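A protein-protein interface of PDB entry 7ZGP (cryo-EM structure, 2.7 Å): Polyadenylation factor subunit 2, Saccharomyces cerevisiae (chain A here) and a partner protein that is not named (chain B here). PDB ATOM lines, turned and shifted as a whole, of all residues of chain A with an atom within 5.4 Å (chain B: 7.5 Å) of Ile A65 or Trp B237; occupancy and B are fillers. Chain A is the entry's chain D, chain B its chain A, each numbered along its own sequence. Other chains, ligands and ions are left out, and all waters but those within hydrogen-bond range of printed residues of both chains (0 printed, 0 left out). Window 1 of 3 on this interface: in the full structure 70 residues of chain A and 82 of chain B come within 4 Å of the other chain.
Ile A65 touches just one residue of chain B: Trp B237 (3.8 Å). Of chain A, only Ile A65, Val A77, Ile A78 and Ala A380 come within 4 Å of Trp B237. Of the printed residues of chain B, Pro A38 touches Glu B1046. Printed residues of chain B within 4 Å of Arg A379: Glu B1046 (3.5 Å). Of the printed residues of chain B, Ile A63 touches Thr B1044 (3.8 Å). Printed residues of chain B within 4 Å of Tyr A61: Arg B338 (3.5 Å). The nearest residue of chain A that does not touch Trp B237 is Val A55 (4.02 Å).
Among the printed residues, merely in contact across the chains: Ala A380 with Trp B237 (3.1 Å), Thr A62 with Thr B1045 (3.2 Å), Val A55 with Ala B238 (3.3 Å), Arg A381 with Gly B239 (3.3 Å), Val A77 with Leu B235 (3.4 Å), Tyr A61 with Arg B338 (3.5 Å), Pro A38 with Glu B1046 (3.7 Å), Val A77 with Trp B237 (3.7 Å), Val A55 with Trp B279 (3.8 Å), Ile A78 with Trp B237 (3.8 Å), Ile A65 with Trp B237 (3.8 Å), Ile A63 with Thr B1044 (3.8 Å), Val A77 with Asn B240 (3.9 Å), Tyr A388 with Thr B242 (3.95 Å), Pro A382 with Gly B239 (3.98 Å) and Ala A380 with Gly B239 (3.996 Å).
The backbone carbonyl oxygen (O) of Gly B239 lies within hydrogen-bond range of the side-chain hydroxyl (OH) of Tyr A388, at 2.5 Å. The side-chain amide oxygen of Asn B240 sits at hydrogen-bond distance from the side-chain hydroxyl of Tyr A388, at 3.4 Å. NH1 of Arg B338 lies within salt-bridge range of OD2 of Asp A64, at 3.4 Å. OE1 of Glu B1046 lies within salt-bridge range of NH2 of Arg A379 (3.5 Å). The side-chain carboxylate of Glu B1046 is in salt-bridge range of the guanidinium group of Arg A381, at 3.99 Å. The guanidinium group (NH1) of Arg A381 is in salt-bridge range of the side-chain carboxylate (OD1) of Asp B1047 (3.0 Å). O of Pro A382 lies close to O of Ala B238, at 3.2 Å.
Hydrophobic or aromatic side chains of chain A that line the printed part of chain B: Pro A38, Val A55, Tyr A61, Ile A63, Ile A65, Val A77, Ile A78, Ala A380 and Tyr A388. Of the 18 printed residues of chain B, 12 touch a printed residue of chain A. Among the printed residues, 23 pairs touch across the chains. Among the printed residues, Asp or Glu carboxylates within 4 Å of a Lys or Arg side-chain nitrogen of the other chain: Asp A64 with Arg B338 (2.3 Å), Arg A379 with Glu B1046 (3.5 Å), Arg A381 with Glu B1046 (3.99 Å) and Arg A381 with Asp B1047 (3.0 Å).
The side-chain amide nitrogen (NE2) of Gln B232 is in hydrogen-bond range of the backbone carbonyl oxygen (O) of Trp B279, 2.5 Å away. NZ of Lys B234 lies close to ND2 of Asn B240, at 3.4 Å. The side-chain amide nitrogen (ND2) of Asn B240 sits at hydrogen-bond distance from the backbone carbonyl oxygen (O) of Leu B235. The side-chain hydroxyl (OG1) of Thr B241 is in hydrogen-bond range of the backbone carbonyl oxygen (O) of Ala B238 (2.9 Å). The backbone carbonyl oxygen (O) of Met A66 lies within hydrogen-bond range of the guanidinium group (NH1) of Arg A379, 2.7 Å away. The backbone carbonyl oxygen (O) of Arg A379 lies within hydrogen-bond range of the guanidinium group (NE) of Arg A381.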
ATOM      1  N   PRO A  38      -9.225 -25.902 -13.498  1.00  0.00           N
ATOM      2  CA  PRO A  38      -8.922 -25.079 -14.676  1.00  0.00           C
ATOM      3  C   PRO A  38     -10.124 -24.869 -15.578  1.00  0.00           C
ATOM      4  O   PRO A  38     -10.272 -23.789 -16.157  1.00  0.00           O
ATOM      5  CB  PRO A  38      -7.813 -25.874 -15.376  1.00  0.00           C
ATOM      6  CG  PRO A  38      -7.147 -26.603 -14.286  1.00  0.00           C
ATOM      7  CD  PRO A  38      -8.226 -26.973 -13.318  1.00  0.00           C
ATOM      8  N   VAL A  55       0.058 -15.987 -18.396  1.00  0.00           N
ATOM      9  CA  VAL A  55       0.652 -16.584 -17.205  1.00  0.00           C
ATOM     10  C   VAL A  55       2.057 -16.027 -17.022  1.00  0.00           C
ATOM     11  O   VAL A  55       2.846 -15.971 -17.972  1.00  0.00           O
ATOM     12  CB  VAL A  55       0.667 -18.116 -17.318  1.00  0.00           C
ATOM     13  CG1 VAL A  55       1.619 -18.721 -16.302  1.00  0.00           C
ATOM     14  CG2 VAL A  55      -0.733 -18.672 -17.140  1.00  0.00           C
ATOM     15  N   TYR A  61       0.406 -18.048 -10.498  1.00  0.00           N
ATOM     16  CA  TYR A  61      -0.181 -17.936 -11.824  1.00  0.00           C
ATOM     17  C   TYR A  61      -0.516 -19.287 -12.438  1.00  0.00           C
ATOM     18  O   TYR A  61      -0.984 -19.330 -13.579  1.00  0.00           O
ATOM     19  CB  TYR A  61       0.761 -17.158 -12.744  1.00  0.00           C
ATOM     20  CG  TYR A  61       0.881 -15.709 -12.344  1.00  0.00           C
ATOM     21  CD1 TYR A  61       1.713 -15.331 -11.301  1.00  0.00           C
ATOM     22  CD2 TYR A  61       0.146 -14.724 -12.987  1.00  0.00           C
ATOM     23  CE1 TYR A  61       1.821 -14.018 -10.919  1.00  0.00           C
ATOM     24  CE2 TYR A  61       0.250 -13.402 -12.608  1.00  0.00           C
ATOM     25  CZ  TYR A  61       1.090 -13.058 -11.572  1.00  0.00           C
ATOM     26  OH  TYR A  61       1.205 -11.749 -11.178  1.00  0.00           O
ATOM     27  N   THR A  62      -0.279 -20.384 -11.717  1.00  0.00           N
ATOM     28  CA  THR A  62      -0.714 -21.689 -12.200  1.00  0.00           C
ATOM     29  C   THR A  62      -2.233 -21.771 -12.275  1.00  0.00           C
ATOM     30  O   THR A  62      -2.776 -22.549 -13.065  1.00  0.00           O
ATOM     31  CB  THR A  62      -0.165 -22.795 -11.300  1.00  0.00           C
ATOM     32  OG1 THR A  62       1.168 -22.462 -10.894  1.00  0.00           O
ATOM     33  CG2 THR A  62      -0.132 -24.113 -12.045  1.00  0.00           C
ATOM     34  N   ILE A  63      -2.934 -20.974 -11.463  1.00  0.00           N
ATOM     35  CA  ILE A  63      -4.386 -20.901 -11.552  1.00  0.00           C
ATOM     36  C   ILE A  63      -4.833 -20.308 -12.881  1.00  0.00           C
ATOM     37  O   ILE A  63      -5.968 -20.546 -13.312  1.00  0.00           O
ATOM     38  CB  ILE A  63      -4.958 -20.093 -10.371  1.00  0.00           C
ATOM     39  CG1 ILE A  63      -6.428 -20.449 -10.142  1.00  0.00           C
ATOM     40  CG2 ILE A  63      -4.793 -18.599 -10.602  1.00  0.00           C
ATOM     41  CD1 ILE A  63      -7.073 -19.683  -9.014  1.00  0.00           C
ATOM     42  N   ASP A  64      -3.971 -19.548 -13.550  1.00  0.00           N
ATOM     43  CA  ASP A  64      -4.292 -18.958 -14.840  1.00  0.00           C
ATOM     44  C   ASP A  64      -3.952 -19.873 -16.007  1.00  0.00           C
ATOM     45  O   ASP A  64      -4.137 -19.474 -17.160  1.00  0.00           O
ATOM     46  CB  ASP A  64      -3.567 -17.619 -15.004  1.00  0.00           C
ATOM     47  CG  ASP A  64      -4.309 -16.472 -14.351  1.00  0.00           C
ATOM     48  OD1 ASP A  64      -5.534 -16.595 -14.148  1.00  0.00           O
ATOM     49  OD2 ASP A  64      -3.671 -15.445 -14.040  1.00  0.00           O
ATOM     50  N   ILE A  65      -3.456 -21.076 -15.740  1.00  0.00           N
ATOM     51  CA  ILE A  65      -3.212 -22.052 -16.796  1.00  0.00           C
ATOM     52  C   ILE A  65      -4.525 -22.760 -17.100  1.00  0.00           C
ATOM     53  O   ILE A  65      -5.103 -23.423 -16.233  1.00  0.00           O
ATOM     54  CB  ILE A  65      -2.122 -23.054 -16.390  1.00  0.00           C
ATOM     55  CG1 ILE A  65      -0.793 -22.334 -16.168  1.00  0.00           C
ATOM     56  CG2 ILE A  65      -1.970 -24.128 -17.453  1.00  0.00           C
ATOM     57  CD1 ILE A  65       0.333 -23.251 -15.761  1.00  0.00           C
ATOM     58  N   MET A  66      -4.992 -22.621 -18.325  1.00  0.00           N
ATOM     59  CA  MET A  66      -6.284 -23.127 -18.751  1.00  0.00           C
ATOM     60  C   MET A  66      -6.176 -24.577 -19.197  1.00  0.00           C
ATOM     61  O   MET A  66      -5.078 -25.086 -19.436  1.00  0.00           O
ATOM     62  CB  MET A  66      -6.830 -22.258 -19.880  1.00  0.00           C
ATOM     63  CG  MET A  66      -7.122 -20.840 -19.438  1.00  0.00           C
ATOM     64  SD  MET A  66      -8.207 -20.811 -18.001  1.00  0.00           S
ATOM     65  CE  MET A  66      -7.907 -19.159 -17.389  1.00  0.00           C
ATOM     66  N   PRO A  67      -7.304 -25.280 -19.292  1.00  0.00           N
ATOM     67  CA  PRO A  67      -7.269 -26.637 -19.824  1.00  0.00           C
ATOM     68  C   PRO A  67      -6.722 -26.644 -21.237  1.00  0.00           C
ATOM     69  O   PRO A  67      -6.837 -25.646 -21.973  1.00  0.00           O
ATOM     70  CB  PRO A  67      -8.743 -27.071 -19.786  1.00  0.00           C
ATOM     71  CG  PRO A  67      -9.524 -25.837 -19.501  1.00  0.00           C
ATOM     72  CD  PRO A  67      -8.625 -24.942 -18.744  1.00  0.00           C
ATOM     73  N   TYR A  71      -6.416 -23.693 -25.580  1.00  0.00           N
ATOM     74  CA  TYR A  71      -5.221 -23.048 -26.105  1.00  0.00           C
ATOM     75  C   TYR A  71      -5.092 -23.336 -27.593  1.00  0.00           C
ATOM     76  O   TYR A  71      -5.024 -24.499 -28.001  1.00  0.00           O
ATOM     77  CB  TYR A  71      -3.977 -23.519 -25.352  1.00  0.00           C
ATOM     78  CG  TYR A  71      -3.861 -22.933 -23.966  1.00  0.00           C
ATOM     79  CD1 TYR A  71      -4.041 -21.575 -23.750  1.00  0.00           C
ATOM     80  CD2 TYR A  71      -3.578 -23.735 -22.872  1.00  0.00           C
ATOM     81  CE1 TYR A  71      -3.939 -21.033 -22.488  1.00  0.00           C
ATOM     82  CE2 TYR A  71      -3.474 -23.200 -21.604  1.00  0.00           C
ATOM     83  CZ  TYR A  71      -3.654 -21.848 -21.418  1.00  0.00           C
ATOM     84  OH  TYR A  71      -3.552 -21.310 -20.158  1.00  0.00           O
ATOM     85  N   VAL A  77       1.946 -23.740 -27.237  1.00  0.00           N
ATOM     86  CA  VAL A  77       3.189 -24.147 -26.589  1.00  0.00           C
ATOM     87  C   VAL A  77       2.939 -24.531 -25.138  1.00  0.00           C
ATOM     88  O   VAL A  77       3.696 -25.315 -24.555  1.00  0.00           O
ATOM     89  CB  VAL A  77       4.247 -23.032 -26.710  1.00  0.00           C
ATOM     90  CG1 VAL A  77       3.868 -21.828 -25.862  1.00  0.00           C
ATOM     91  CG2 VAL A  77       5.624 -23.553 -26.331  1.00  0.00           C
ATOM     92  N   ILE A  78       1.878 -23.993 -24.532  1.00  0.00           N
ATOM     93  CA  ILE A  78       1.538 -24.360 -23.162  1.00  0.00           C
ATOM     94  C   ILE A  78       1.141 -25.825 -23.084  1.00  0.00           C
ATOM     95  O   ILE A  78       1.365 -26.484 -22.062  1.00  0.00           O
ATOM     96  CB  ILE A  78       0.424 -23.439 -22.627  1.00  0.00           C
ATOM     97  CG1 ILE A  78       0.760 -21.976 -22.920  1.00  0.00           C
ATOM     98  CG2 ILE A  78       0.221 -23.653 -21.136  1.00  0.00           C
ATOM     99  CD1 ILE A  78      -0.135 -20.984 -22.209  1.00  0.00           C
ATOM    100  N   ARG A 379       1.782 -30.909 -18.313  1.00  0.00           N
ATOM    101  CA  ARG A 379       2.279 -29.661 -18.864  1.00  0.00           C
ATOM    102  C   ARG A 379       3.215 -28.970 -17.876  1.00  0.00           C
ATOM    103  O   ARG A 379       3.180 -29.212 -16.667  1.00  0.00           O
ATOM    104  CB  ARG A 379       1.117 -28.742 -19.234  1.00  0.00           C
ATOM    105  CG  ARG A 379       0.264 -29.272 -20.374  1.00  0.00           C
ATOM    106  CD  ARG A 379      -0.891 -28.342 -20.688  1.00  0.00           C
ATOM    107  NE  ARG A 379      -1.855 -28.274 -19.597  1.00  0.00           N
ATOM    108  CZ  ARG A 379      -2.849 -27.400 -19.535  1.00  0.00           C
ATOM    109  NH1 ARG A 379      -3.038 -26.501 -20.485  1.00  0.00           N
ATOM    110  NH2 ARG A 379      -3.670 -27.427 -18.491  1.00  0.00           N
ATOM    111  N   ALA A 380       4.067 -28.104 -18.414  1.00  0.00           N
ATOM    112  CA  ALA A 380       5.035 -27.388 -17.597  1.00  0.00           C
ATOM    113  C   ALA A 380       4.341 -26.384 -16.684  1.00  0.00           C
ATOM    114  O   ALA A 380       3.256 -25.880 -16.983  1.00  0.00           O
ATOM    115  CB  ALA A 380       6.053 -26.670 -18.480  1.00  0.00           C
ATOM    116  N   ARG A 381       4.977 -26.104 -15.557  1.00  0.00           N
ATOM    117  CA  ARG A 381       4.490 -25.134 -14.592  1.00  0.00           C
ATOM    118  C   ARG A 381       5.131 -23.775 -14.839  1.00  0.00           C
ATOM    119  O   ARG A 381       6.209 -23.688 -15.435  1.00  0.00           O
ATOM    120  CB  ARG A 381       4.789 -25.619 -13.174  1.00  0.00           C
ATOM    121  CG  ARG A 381       4.413 -27.073 -12.918  1.00  0.00           C
ATOM    122  CD  ARG A 381       2.908 -27.268 -12.753  1.00  0.00           C
ATOM    123  NE  ARG A 381       2.199 -27.235 -14.027  1.00  0.00           N
ATOM    124  CZ  ARG A 381       0.880 -27.202 -14.153  1.00  0.00           C
ATOM    125  NH1 ARG A 381       0.083 -27.222 -13.098  1.00  0.00           N
ATOM    126  NH2 ARG A 381       0.347 -27.150 -15.371  1.00  0.00           N
ATOM    127  N   PRO A 382       4.481 -22.684 -14.410  1.00  0.00           N
ATOM    128  CA  PRO A 382       5.049 -21.351 -14.687  1.00  0.00           C
ATOM    129  C   PRO A 382       6.455 -21.171 -14.150  1.00  0.00           C
ATOM    130  O   PRO A 382       7.295 -20.548 -14.812  1.00  0.00           O
ATOM    131  CB  PRO A 382       4.054 -20.399 -14.005  1.00  0.00           C
ATOM    132  CG  PRO A 382       2.807 -21.187 -13.840  1.00  0.00           C
ATOM    133  CD  PRO A 382       3.229 -22.600 -13.641  1.00  0.00           C
ATOM    134  N   TYR A 388      13.056 -29.150 -16.983  1.00  0.00           N
ATOM    135  CA  TYR A 388      14.049 -29.491 -18.000  1.00  0.00           C
ATOM    136  C   TYR A 388      15.397 -29.864 -17.391  1.00  0.00           C
ATOM    137  O   TYR A 388      16.433 -29.770 -18.057  1.00  0.00           O
ATOM    138  CB  TYR A 388      14.208 -28.354 -19.016  1.00  0.00           C
ATOM    139  CG  TYR A 388      12.895 -27.692 -19.373  1.00  0.00           C
ATOM    140  CD1 TYR A 388      11.988 -28.320 -20.216  1.00  0.00           C
ATOM    141  CD2 TYR A 388      12.557 -26.450 -18.857  1.00  0.00           C
ATOM    142  CE1 TYR A 388      10.785 -27.724 -20.540  1.00  0.00           C
ATOM    143  CE2 TYR A 388      11.357 -25.846 -19.177  1.00  0.00           C
ATOM    144  CZ  TYR A 388      10.475 -26.487 -20.018  1.00  0.00           C
ATOM    145  OH  TYR A 388       9.278 -25.890 -20.338  1.00  0.00           O
ATOM    146  N   GLN B 232       7.407 -14.786 -33.126  1.00  0.00           N
ATOM    147  CA  GLN B 232       8.248 -15.677 -32.327  1.00  0.00           C
ATOM    148  C   GLN B 232       8.503 -16.954 -33.113  1.00  0.00           C
ATOM    149  O   GLN B 232       7.630 -17.837 -33.162  1.00  0.00           O
ATOM    150  CB  GLN B 232       7.583 -16.001 -30.991  1.00  0.00           C
ATOM    151  CG  GLN B 232       7.956 -15.068 -29.863  1.00  0.00           C
ATOM    152  CD  GLN B 232       7.416 -15.531 -28.528  1.00  0.00           C
ATOM    153  OE1 GLN B 232       6.915 -16.647 -28.402  1.00  0.00           O
ATOM    154  NE2 GLN B 232       7.508 -14.672 -27.524  1.00  0.00           N
ATOM    155  N   LYS B 234      10.243 -19.447 -32.286  1.00  0.00           N
ATOM    156  CA  LYS B 234      10.099 -20.508 -31.300  1.00  0.00           C
ATOM    157  C   LYS B 234       9.178 -20.008 -30.197  1.00  0.00           C
ATOM    158  O   LYS B 234       9.521 -19.059 -29.484  1.00  0.00           O
ATOM    159  CB  LYS B 234      11.459 -20.919 -30.733  1.00  0.00           C
ATOM    160  CG  LYS B 234      11.397 -22.028 -29.704  1.00  0.00           C
ATOM    161  CD  LYS B 234      12.788 -22.404 -29.226  1.00  0.00           C
ATOM    162  CE  LYS B 234      12.731 -23.500 -28.175  1.00  0.00           C
ATOM    163  NZ  LYS B 234      11.932 -23.091 -26.990  1.00  0.00           N
ATOM    164  N   LEU B 235       8.014 -20.638 -30.064  1.00  0.00           N
ATOM    165  CA  LEU B 235       7.015 -20.181 -29.108  1.00  0.00           C
ATOM    166  C   LEU B 235       7.516 -20.358 -27.681  1.00  0.00           C
ATOM    167  O   LEU B 235       8.058 -21.408 -27.325  1.00  0.00           O
ATOM    168  CB  LEU B 235       5.709 -20.944 -29.304  1.00  0.00           C
ATOM    169  CG  LEU B 235       4.957 -20.684 -30.607  1.00  0.00           C
ATOM    170  CD1 LEU B 235       3.610 -21.374 -30.572  1.00  0.00           C
ATOM    171  CD2 LEU B 235       4.792 -19.195 -30.828  1.00  0.00           C
ATOM    172  N   VAL B 236       7.332 -19.323 -26.863  1.00  0.00           N
ATOM    173  CA  VAL B 236       7.805 -19.311 -25.484  1.00  0.00           C
ATOM    174  C   VAL B 236       6.708 -18.753 -24.592  1.00  0.00           C
ATOM    175  O   VAL B 236       6.097 -17.730 -24.916  1.00  0.00           O
ATOM    176  CB  VAL B 236       9.096 -18.484 -25.333  1.00  0.00           C
ATOM    177  CG1 VAL B 236       9.476 -18.343 -23.869  1.00  0.00           C
ATOM    178  CG2 VAL B 236      10.220 -19.130 -26.109  1.00  0.00           C
ATOM    179  N   TRP B 237       6.454 -19.428 -23.472  1.00  0.00           N
ATOM    180  CA  TRP B 237       5.547 -18.919 -22.452  1.00  0.00           C
ATOM    181  C   TRP B 237       6.254 -18.920 -21.103  1.00  0.00           C
ATOM    182  O   TRP B 237       7.475 -19.085 -21.045  1.00  0.00           O
ATOM    183  CB  TRP B 237       4.257 -19.739 -22.407  1.00  0.00           C
ATOM    184  CG  TRP B 237       4.412 -21.115 -21.842  1.00  0.00           C
ATOM    185  CD1 TRP B 237       5.145 -22.138 -22.365  1.00  0.00           C
ATOM    186  CD2 TRP B 237       3.808 -21.622 -20.648  1.00  0.00           C
ATOM    187  NE1 TRP B 237       5.039 -23.251 -21.568  1.00  0.00           N
ATOM    188  CE2 TRP B 237       4.223 -22.960 -20.507  1.00  0.00           C
ATOM    189  CE3 TRP B 237       2.958 -21.075 -19.684  1.00  0.00           C
ATOM    190  CZ2 TRP B 237       3.818 -23.756 -19.441  1.00  0.00           C
ATOM    191  CZ3 TRP B 237       2.558 -21.867 -18.627  1.00  0.00           C
ATOM    192  CH2 TRP B 237       2.988 -23.193 -18.514  1.00  0.00           C
ATOM    193  N   ALA B 238       5.501 -18.727 -20.017  1.00  0.00           N
ATOM    194  CA  ALA B 238       6.117 -18.627 -18.696  1.00  0.00           C
ATOM    195  C   ALA B 238       6.900 -19.886 -18.345  1.00  0.00           C
ATOM    196  O   ALA B 238       8.011 -19.804 -17.808  1.00  0.00           O
ATOM    197  CB  ALA B 238       5.049 -18.352 -17.640  1.00  0.00           C
ATOM    198  N   GLY B 239       6.344 -21.056 -18.644  1.00  0.00           N
ATOM    199  CA  GLY B 239       7.021 -22.307 -18.377  1.00  0.00           C
ATOM    200  C   GLY B 239       8.096 -22.683 -19.368  1.00  0.00           C
ATOM    201  O   GLY B 239       8.682 -23.762 -19.256  1.00  0.00           O
ATOM    202  N   ASN B 240       8.372 -21.819 -20.341  1.00  0.00           N
ATOM    203  CA  ASN B 240       9.363 -22.082 -21.373  1.00  0.00           C
ATOM    204  C   ASN B 240      10.512 -21.084 -21.368  1.00  0.00           C
ATOM    205  O   ASN B 240      11.430 -21.218 -22.186  1.00  0.00           O
ATOM    206  CB  ASN B 240       8.691 -22.081 -22.753  1.00  0.00           C
ATOM    207  CG  ASN B 240       9.267 -23.123 -23.683  1.00  0.00           C
ATOM    208  OD1 ASN B 240       9.769 -24.156 -23.243  1.00  0.00           O
ATOM    209  ND2 ASN B 240       9.198 -22.858 -24.981  1.00  0.00           N
ATOM    210  N   THR B 241      10.490 -20.090 -20.476  1.00  0.00           N
ATOM    211  CA  THR B 241      11.444 -18.988 -20.554  1.00  0.00           C
ATOM    212  C   THR B 241      12.852 -19.407 -20.154  1.00  0.00           C
ATOM    213  O   THR B 241      13.829 -18.890 -20.709  1.00  0.00           O
ATOM    214  CB  THR B 241      10.978 -17.831 -19.672  1.00  0.00           C
ATOM    215  OG1 THR B 241      10.434 -18.349 -18.452  1.00  0.00           O
ATOM    216  CG2 THR B 241       9.913 -17.023 -20.383  1.00  0.00           C
ATOM    217  N   THR B 242      12.983 -20.328 -19.197  1.00  0.00           N
ATOM    218  CA  THR B 242      14.304 -20.673 -18.680  1.00  0.00           C
ATOM    219  C   THR B 242      15.168 -21.366 -19.725  1.00  0.00           C
ATOM    220  O   THR B 242      16.400 -21.284 -19.658  1.00  0.00           O
ATOM    221  CB  THR B 242      14.172 -21.554 -17.437  1.00  0.00           C
ATOM    222  OG1 THR B 242      13.480 -22.762 -17.777  1.00  0.00           O
ATOM    223  CG2 THR B 242      13.405 -20.825 -16.347  1.00  0.00           C
ATOM    224  N   SER B 244      14.678 -20.882 -23.131  1.00  0.00           N
ATOM    225  CA  SER B 244      14.558 -20.161 -24.395  1.00  0.00           C
ATOM    226  C   SER B 244      14.641 -18.673 -24.094  1.00  0.00           C
ATOM    227  O   SER B 244      13.726 -18.110 -23.486  1.00  0.00           O
ATOM    228  CB  SER B 244      13.254 -20.509 -25.102  1.00  0.00           C
ATOM    229  OG  SER B 244      13.141 -21.905 -25.315  1.00  0.00           O
ATOM    230  N   PRO B 247      13.117 -14.794 -27.518  1.00  0.00           N
ATOM    231  CA  PRO B 247      12.674 -15.479 -28.739  1.00  0.00           C
ATOM    232  C   PRO B 247      11.994 -14.565 -29.746  1.00  0.00           C
ATOM    233  O   PRO B 247      11.964 -14.870 -30.942  1.00  0.00           O
ATOM    234  CB  PRO B 247      11.694 -16.522 -28.198  1.00  0.00           C
ATOM    235  CG  PRO B 247      11.089 -15.846 -27.007  1.00  0.00           C
ATOM    236  CD  PRO B 247      12.131 -14.916 -26.432  1.00  0.00           C
ATOM    237  N   TRP B 279      10.098 -12.274 -24.550  1.00  0.00           N
ATOM    238  CA  TRP B 279       9.096 -13.241 -24.988  1.00  0.00           C
ATOM    239  C   TRP B 279       7.678 -12.690 -24.905  1.00  0.00           C
ATOM    240  O   TRP B 279       6.803 -13.128 -25.660  1.00  0.00           O
ATOM    241  CB  TRP B 279       9.203 -14.513 -24.149  1.00  0.00           C
ATOM    242  CG  TRP B 279       8.953 -14.280 -22.690  1.00  0.00           C
ATOM    243  CD1 TRP B 279       9.848 -13.822 -21.770  1.00  0.00           C
ATOM    244  CD2 TRP B 279       7.726 -14.493 -21.984  1.00  0.00           C
ATOM    245  NE1 TRP B 279       9.255 -13.736 -20.535  1.00  0.00           N
ATOM    246  CE2 TRP B 279       7.952 -14.143 -20.640  1.00  0.00           C
ATOM    247  CE3 TRP B 279       6.458 -14.947 -22.359  1.00  0.00           C
ATOM    248  CZ2 TRP B 279       6.958 -14.231 -19.669  1.00  0.00           C
ATOM    249  CZ3 TRP B 279       5.474 -15.034 -21.395  1.00  0.00           C
ATOM    250  CH2 TRP B 279       5.729 -14.678 -20.065  1.00  0.00           C
ATOM    251  N   ARG B 338      -1.446  -7.795 -19.407  1.00  0.00           N
ATOM    252  CA  ARG B 338      -1.643  -9.235 -19.516  1.00  0.00           C
ATOM    253  C   ARG B 338      -2.624  -9.622 -20.613  1.00  0.00           C
ATOM    254  O   ARG B 338      -2.833 -10.816 -20.842  1.00  0.00           O
ATOM    255  CB  ARG B 338      -2.119  -9.801 -18.175  1.00  0.00           C
ATOM    256  CG  ARG B 338      -1.053  -9.810 -17.096  1.00  0.00           C
ATOM    257  CD  ARG B 338      -1.562 -10.441 -15.812  1.00  0.00           C
ATOM    258  NE  ARG B 338      -1.647 -11.891 -15.917  1.00  0.00           N
ATOM    259  CZ  ARG B 338      -2.343 -12.664 -15.095  1.00  0.00           C
ATOM    260  NH1 ARG B 338      -3.032 -12.155 -14.087  1.00  0.00           N
ATOM    261  NH2 ARG B 338      -2.348 -13.978 -15.289  1.00  0.00           N
ATOM    262  N   THR B1044      -9.024 -23.526  -7.918  1.00  0.00           N
ATOM    263  CA  THR B1044      -7.628 -23.670  -7.540  1.00  0.00           C
ATOM    264  C   THR B1044      -6.862 -24.186  -8.754  1.00  0.00           C
ATOM    265  O   THR B1044      -7.358 -24.159  -9.883  1.00  0.00           O
ATOM    266  CB  THR B1044      -7.478 -24.594  -6.323  1.00  0.00           C
ATOM    267  OG1 THR B1044      -8.293 -25.758  -6.500  1.00  0.00           O
ATOM    268  CG2 THR B1044      -7.889 -23.880  -5.046  1.00  0.00           C
ATOM    269  N   THR B1045      -5.639 -24.648  -8.521  1.00  0.00           N
ATOM    270  CA  THR B1045      -4.781 -25.086  -9.608  1.00  0.00           C
ATOM    271  C   THR B1045      -5.120 -26.516 -10.030  1.00  0.00           C
ATOM    272  O   THR B1045      -5.907 -27.218  -9.392  1.00  0.00           O
ATOM    273  CB  THR B1045      -3.311 -24.987  -9.205  1.00  0.00           C
ATOM    274  OG1 THR B1045      -2.487 -25.386 -10.304  1.00  0.00           O
ATOM    275  CG2 THR B1045      -3.021 -25.878  -8.012  1.00  0.00           C
ATOM    276  N   GLU B1046      -4.511 -26.936 -11.140  1.00  0.00           N
ATOM    277  CA  GLU B1046      -4.719 -28.289 -11.644  1.00  0.00           C
ATOM    278  C   GLU B1046      -4.080 -29.334 -10.737  1.00  0.00           C
ATOM    279  O   GLU B1046      -4.568 -30.466 -10.655  1.00  0.00           O
ATOM    280  CB  GLU B1046      -4.166 -28.394 -13.067  1.00  0.00           C
ATOM    281  CG  GLU B1046      -4.010 -29.806 -13.603  1.00  0.00           C
ATOM    282  CD  GLU B1046      -3.594 -29.832 -15.061  1.00  0.00           C
ATOM    283  OE1 GLU B1046      -4.466 -29.639 -15.933  1.00  0.00           O
ATOM    284  OE2 GLU B1046      -2.395 -30.045 -15.336  1.00  0.00           O
ATOM    285  N   ASP B1047      -3.008 -28.967 -10.031  1.00  0.00           N
ATOM    286  CA  ASP B1047      -2.243 -29.954  -9.276  1.00  0.00           C
ATOM    287  C   ASP B1047      -2.954 -30.355  -7.988  1.00  0.00           C
ATOM    288  O   ASP B1047      -2.828 -31.499  -7.536  1.00  0.00           O
ATOM    289  CB  ASP B1047      -0.850 -29.408  -8.974  1.00  0.00           C
ATOM    290  CG  ASP B1047      -0.117 -28.970 -10.225  1.00  0.00           C
ATOM    291  OD1 ASP B1047      -0.306 -29.611 -11.281  1.00  0.00           O
ATOM    292  OD2 ASP B1047       0.646 -27.984 -10.156  1.00  0.00           O
